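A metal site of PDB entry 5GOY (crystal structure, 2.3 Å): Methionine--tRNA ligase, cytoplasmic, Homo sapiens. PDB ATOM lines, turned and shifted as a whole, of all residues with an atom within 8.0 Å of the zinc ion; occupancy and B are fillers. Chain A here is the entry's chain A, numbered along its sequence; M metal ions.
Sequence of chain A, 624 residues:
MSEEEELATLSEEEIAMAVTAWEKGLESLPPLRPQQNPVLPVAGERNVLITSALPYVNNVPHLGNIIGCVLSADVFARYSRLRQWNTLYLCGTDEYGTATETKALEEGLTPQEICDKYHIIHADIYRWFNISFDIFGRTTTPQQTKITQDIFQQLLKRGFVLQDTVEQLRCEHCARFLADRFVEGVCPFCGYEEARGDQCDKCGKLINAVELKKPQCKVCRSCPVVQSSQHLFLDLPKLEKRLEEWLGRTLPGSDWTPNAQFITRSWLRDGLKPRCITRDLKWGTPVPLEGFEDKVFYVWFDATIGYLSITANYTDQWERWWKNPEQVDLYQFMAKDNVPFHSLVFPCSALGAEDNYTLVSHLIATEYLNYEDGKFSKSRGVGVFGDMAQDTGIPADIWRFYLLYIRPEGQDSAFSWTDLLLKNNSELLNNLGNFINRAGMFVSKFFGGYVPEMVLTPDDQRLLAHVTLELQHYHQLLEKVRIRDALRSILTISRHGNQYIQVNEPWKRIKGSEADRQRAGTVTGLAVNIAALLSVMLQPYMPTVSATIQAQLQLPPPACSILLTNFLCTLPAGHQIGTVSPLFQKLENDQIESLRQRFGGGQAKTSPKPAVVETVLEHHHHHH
The zinc ion is bound by the side-chain sulfur of Cys 220 (2.3 Å), the side-chain sulfur of Cys 171 (2.3 Å), the side-chain sulfur of Cys 217 (2.4 Å) and the side-chain sulfur of Cys 174 (2.6 Å).
The side-chain sulfur (SG) of Cys 220 sits close to the side-chain hydroxyl (OG) of Ser 222.
OG of Ser 222 sits close to SG of Cys 171 (3.1 Å).
The side-chain sulfur of Cys 171 sits close to the backbone NH of His 173 (3.5 Å).
The backbone NH (N) of Cys 171 lies within hydrogen-bond range of the backbone carbonyl oxygen (O) of Arg 176 (3.1 Å).
The backbone NH (N) of Cys 217 is in hydrogen-bond range of the backbone carbonyl oxygen (O) of Ser 222 (3.1 Å).
The side-chain sulfur (SG) of Cys 217 sits close to the backbone NH (N) of Val 219, 3.6 Å away.
Residues that only touch the zinc ion: Ser 222 (3.8 Å).
Five residues have an atom within 4 Å of the zinc ion: Cys 171, Cys 174, Cys 217, Cys 220 and Ser 222.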
ATOM      1  N   ARG A 170      -7.676  -9.752   9.209  1.00  0.00           N
ATOM      2  CA  ARG A 170      -8.068  -8.775   8.211  1.00  0.00           C
ATOM      3  C   ARG A 170      -7.241  -7.504   8.326  1.00  0.00           C
ATOM      4  O   ARG A 170      -7.128  -6.916   9.401  1.00  0.00           O
ATOM      5  CB  ARG A 170      -9.558  -8.440   8.327  1.00  0.00           C
ATOM      6  CG  ARG A 170     -10.018  -7.380   7.340  1.00  0.00           C
ATOM      7  CD  ARG A 170     -11.520  -7.198   7.350  1.00  0.00           C
ATOM      8  NE  ARG A 170     -11.958  -6.186   6.399  1.00  0.00           N
ATOM      9  CZ  ARG A 170     -12.252  -6.434   5.124  1.00  0.00           C
ATOM     10  NH1 ARG A 170     -12.157  -7.659   4.648  1.00  0.00           N
ATOM     11  NH2 ARG A 170     -12.636  -5.442   4.327  1.00  0.00           N
ATOM     12  N   CYS A 171      -6.643  -7.092   7.212  1.00  0.00           N
ATOM     13  CA  CYS A 171      -5.939  -5.825   7.144  1.00  0.00           C
ATOM     14  C   CYS A 171      -6.915  -4.696   6.839  1.00  0.00           C
ATOM     15  O   CYS A 171      -7.500  -4.637   5.751  1.00  0.00           O
ATOM     16  CB  CYS A 171      -4.838  -5.872   6.087  1.00  0.00           C
ATOM     17  SG  CYS A 171      -4.070  -4.280   5.766  1.00  0.00           S
ATOM     18  N   GLU A 172      -7.096  -3.796   7.801  1.00  0.00           N
ATOM     19  CA  GLU A 172      -8.073  -2.716   7.672  1.00  0.00           C
ATOM     20  C   GLU A 172      -7.600  -1.638   6.693  1.00  0.00           C
ATOM     21  O   GLU A 172      -8.419  -0.860   6.201  1.00  0.00           O
ATOM     22  CB  GLU A 172      -8.347  -2.094   9.043  1.00  0.00           C
ATOM     23  CG  GLU A 172      -9.218  -2.966   9.931  1.00  0.00           C
ATOM     24  CD  GLU A 172      -9.130  -2.591  11.395  1.00  0.00           C
ATOM     25  OE1 GLU A 172      -8.089  -2.076  11.821  1.00  0.00           O
ATOM     26  OE2 GLU A 172     -10.120  -2.824  12.120  1.00  0.00           O
ATOM     27  N   HIS A 173      -6.309  -1.614   6.405  1.00  0.00           N
ATOM     28  CA  HIS A 173      -5.775  -0.657   5.450  1.00  0.00           C
ATOM     29  C   HIS A 173      -5.992  -1.147   4.019  1.00  0.00           C
ATOM     30  O   HIS A 173      -6.434  -0.394   3.159  1.00  0.00           O
ATOM     31  CB  HIS A 173      -4.290  -0.407   5.699  1.00  0.00           C
ATOM     32  CG  HIS A 173      -3.753   0.803   4.994  1.00  0.00           C
ATOM     33  ND1 HIS A 173      -2.894   0.730   3.920  1.00  0.00           N
ATOM     34  CD2 HIS A 173      -3.969   2.127   5.198  1.00  0.00           C
ATOM     35  CE1 HIS A 173      -2.603   1.947   3.503  1.00  0.00           C
ATOM     36  NE2 HIS A 173      -3.237   2.810   4.262  1.00  0.00           N
ATOM     37  N   CYS A 174      -5.676  -2.413   3.770  1.00  0.00           N
ATOM     38  CA  CYS A 174      -5.913  -3.017   2.469  1.00  0.00           C
ATOM     39  C   CYS A 174      -7.395  -3.339   2.267  1.00  0.00           C
ATOM     40  O   CYS A 174      -7.827  -3.602   1.157  1.00  0.00           O
ATOM     41  CB  CYS A 174      -5.068  -4.278   2.288  1.00  0.00           C
ATOM     42  SG  CYS A 174      -3.318  -3.987   1.990  1.00  0.00           S
ATOM     43  N   ALA A 175      -8.143  -3.307   3.366  1.00  0.00           N
ATOM     44  CA  ALA A 175      -9.570  -3.632   3.369  1.00  0.00           C
ATOM     45  C   ALA A 175      -9.842  -4.997   2.745  1.00  0.00           C
ATOM     46  O   ALA A 175     -10.608  -5.115   1.783  1.00  0.00           O
ATOM     47  CB  ALA A 175     -10.366  -2.554   2.640  1.00  0.00           C
ATOM     48  N   ARG A 176      -9.215  -6.027   3.296  1.00  0.00           N
ATOM     49  CA  ARG A 176      -9.376  -7.380   2.797  1.00  0.00           C
ATOM     50  C   ARG A 176      -8.933  -8.415   3.833  1.00  0.00           C
ATOM     51  O   ARG A 176      -8.166  -8.098   4.745  1.00  0.00           O
ATOM     52  CB  ARG A 176      -8.573  -7.576   1.506  1.00  0.00           C
ATOM     53  CG  ARG A 176      -7.081  -7.695   1.738  1.00  0.00           C
ATOM     54  CD  ARG A 176      -6.336  -7.991   0.453  1.00  0.00           C
ATOM     55  NE  ARG A 176      -4.935  -8.298   0.720  1.00  0.00           N
ATOM     56  CZ  ARG A 176      -4.009  -8.478  -0.223  1.00  0.00           C
ATOM     57  NH1 ARG A 176      -4.337  -8.376  -1.512  1.00  0.00           N
ATOM     58  NH2 ARG A 176      -2.765  -8.758   0.121  1.00  0.00           N
ATOM     59  N   LEU A 178      -6.721 -11.674   4.809  1.00  0.00           N
ATOM     60  CA  LEU A 178      -5.372 -12.030   4.393  1.00  0.00           C
ATOM     61  C   LEU A 178      -5.159 -13.529   4.248  1.00  0.00           C
ATOM     62  O   LEU A 178      -5.629 -14.312   5.065  1.00  0.00           O
ATOM     63  CB  LEU A 178      -4.346 -11.472   5.388  1.00  0.00           C
ATOM     64  CG  LEU A 178      -3.743 -10.102   5.079  1.00  0.00           C
ATOM     65  CD1 LEU A 178      -4.822  -9.092   4.738  1.00  0.00           C
ATOM     66  CD2 LEU A 178      -2.901  -9.627   6.252  1.00  0.00           C
ATOM     67  N   PHE A 182       0.342 -13.910   2.827  1.00  0.00           N
ATOM     68  CA  PHE A 182       0.393 -12.450   2.842  1.00  0.00           C
ATOM     69  C   PHE A 182       0.588 -11.906   4.258  1.00  0.00           C
ATOM     70  O   PHE A 182       0.617 -10.699   4.469  1.00  0.00           O
ATOM     71  CB  PHE A 182      -0.879 -11.866   2.241  1.00  0.00           C
ATOM     72  CG  PHE A 182      -1.010 -12.097   0.756  1.00  0.00           C
ATOM     73  CD1 PHE A 182       0.109 -12.325  -0.027  1.00  0.00           C
ATOM     74  CD2 PHE A 182      -2.256 -12.070   0.148  1.00  0.00           C
ATOM     75  CE1 PHE A 182      -0.006 -12.541  -1.382  1.00  0.00           C
ATOM     76  CE2 PHE A 182      -2.382 -12.288  -1.215  1.00  0.00           C
ATOM     77  CZ  PHE A 182      -1.256 -12.520  -1.983  1.00  0.00           C
ATOM     78  N   GLN A 216       1.714  -9.012  10.710  1.00  0.00           N
ATOM     79  CA  GLN A 216       1.884  -7.947   9.729  1.00  0.00           C
ATOM     80  C   GLN A 216       1.324  -8.336   8.367  1.00  0.00           C
ATOM     81  O   GLN A 216       1.466  -9.477   7.941  1.00  0.00           O
ATOM     82  CB  GLN A 216       3.362  -7.577   9.569  1.00  0.00           C
ATOM     83  CG  GLN A 216       3.895  -6.584  10.564  1.00  0.00           C
ATOM     84  CD  GLN A 216       5.258  -6.054  10.184  1.00  0.00           C
ATOM     85  OE1 GLN A 216       6.243  -6.795  10.154  1.00  0.00           O
ATOM     86  NE2 GLN A 216       5.331  -4.766   9.861  1.00  0.00           N
ATOM     87  N   CYS A 217       0.717  -7.372   7.681  1.00  0.00           N
ATOM     88  CA  CYS A 217       0.336  -7.566   6.286  1.00  0.00           C
ATOM     89  C   CYS A 217       1.526  -7.264   5.391  1.00  0.00           C
ATOM     90  O   CYS A 217       1.953  -6.124   5.292  1.00  0.00           O
ATOM     91  CB  CYS A 217      -0.842  -6.662   5.911  1.00  0.00           C
ATOM     92  SG  CYS A 217      -1.213  -6.625   4.140  1.00  0.00           S
ATOM     93  N   LYS A 218       2.070  -8.291   4.739  1.00  0.00           N
ATOM     94  CA  LYS A 218       3.307  -8.126   3.965  1.00  0.00           C
ATOM     95  C   LYS A 218       3.176  -7.146   2.788  1.00  0.00           C
ATOM     96  O   LYS A 218       4.168  -6.864   2.114  1.00  0.00           O
ATOM     97  CB  LYS A 218       3.805  -9.484   3.462  1.00  0.00           C
ATOM     98  CG  LYS A 218       4.900 -10.076   4.336  1.00  0.00           C
ATOM     99  CD  LYS A 218       5.792 -11.029   3.557  1.00  0.00           C
ATOM    100  CE  LYS A 218       7.082 -11.314   4.311  1.00  0.00           C
ATOM    101  NZ  LYS A 218       7.848 -10.054   4.584  1.00  0.00           N
ATOM    102  N   VAL A 219       1.971  -6.640   2.561  1.00  0.00           N
ATOM    103  CA  VAL A 219       1.741  -5.670   1.494  1.00  0.00           C
ATOM    104  C   VAL A 219       1.955  -4.237   1.965  1.00  0.00           C
ATOM    105  O   VAL A 219       2.741  -3.498   1.371  1.00  0.00           O
ATOM    106  CB  VAL A 219       0.319  -5.801   0.913  1.00  0.00           C
ATOM    107  CG1 VAL A 219       0.065  -4.712  -0.117  1.00  0.00           C
ATOM    108  CG2 VAL A 219       0.125  -7.180   0.311  1.00  0.00           C
ATOM    109  N   CYS A 220       1.261  -3.854   3.031  1.00  0.00           N
ATOM    110  CA  CYS A 220       1.325  -2.475   3.528  1.00  0.00           C
ATOM    111  C   CYS A 220       2.011  -2.393   4.886  1.00  0.00           C
ATOM    112  O   CYS A 220       2.182  -1.296   5.442  1.00  0.00           O
ATOM    113  CB  CYS A 220      -0.082  -1.883   3.632  1.00  0.00           C
ATOM    114  SG  CYS A 220      -1.091  -2.657   4.907  1.00  0.00           S
ATOM    115  N   ARG A 221       2.393  -3.546   5.422  1.00  0.00           N
ATOM    116  CA  ARG A 221       3.107  -3.641   6.700  1.00  0.00           C
ATOM    117  C   ARG A 221       2.294  -3.112   7.893  1.00  0.00           C
ATOM    118  O   ARG A 221       2.874  -2.752   8.915  1.00  0.00           O
ATOM    119  CB  ARG A 221       4.452  -2.913   6.609  1.00  0.00           C
ATOM    120  CG  ARG A 221       5.513  -3.661   5.818  1.00  0.00           C
ATOM    121  CD  ARG A 221       6.055  -4.836   6.619  1.00  0.00           C
ATOM    122  NE  ARG A 221       7.246  -5.416   6.003  1.00  0.00           N
ATOM    123  CZ  ARG A 221       8.183  -6.083   6.681  1.00  0.00           C
ATOM    124  NH1 ARG A 221       8.075  -6.237   7.988  1.00  0.00           N
ATOM    125  NH2 ARG A 221       9.235  -6.582   6.039  1.00  0.00           N
ATOM    126  N   SER A 222       0.971  -3.089   7.761  1.00  0.00           N
ATOM    127  CA  SER A 222       0.126  -2.670   8.869  1.00  0.00           C
ATOM    128  C   SER A 222      -0.206  -3.852   9.773  1.00  0.00           C
ATOM    129  O   SER A 222       0.249  -4.971   9.514  1.00  0.00           O
ATOM    130  CB  SER A 222      -1.173  -2.016   8.374  1.00  0.00           C
ATOM    131  OG  SER A 222      -2.034  -2.966   7.775  1.00  0.00           O
ATOM    132  N   CYS A 223      -0.981  -3.612  10.818  1.00  0.00           N
ATOM    133  CA  CYS A 223      -1.342  -4.652  11.767  1.00  0.00           C
ATOM    134  C   CYS A 223      -2.752  -5.170  11.531  1.00  0.00           C
ATOM    135  O   CYS A 223      -3.727  -4.462  11.789  1.00  0.00           O
ATOM    136  CB  CYS A 223      -1.215  -4.145  13.203  1.00  0.00           C
ATOM    137  SG  CYS A 223       0.466  -3.678  13.664  1.00  0.00           S
ATOM    138  N   PRO A 224      -2.867  -6.419  11.040  1.00  0.00           N
ATOM    139  CA  PRO A 224      -4.164  -7.061  10.833  1.00  0.00           C
ATOM    140  C   PRO A 224      -4.853  -7.342  12.162  1.00  0.00           C
ATOM    141  O   PRO A 224      -4.185  -7.576  13.168  1.00  0.00           O
ATOM    142  CB  PRO A 224      -3.801  -8.372  10.118  1.00  0.00           C
ATOM    143  CG  PRO A 224      -2.430  -8.157   9.580  1.00  0.00           C
ATOM    144  CD  PRO A 224      -1.757  -7.250  10.564  1.00  0.00           C
HETATM  145 ZN    ZN M   1      -2.291  -4.530   4.295  1.00  0.00          ZN
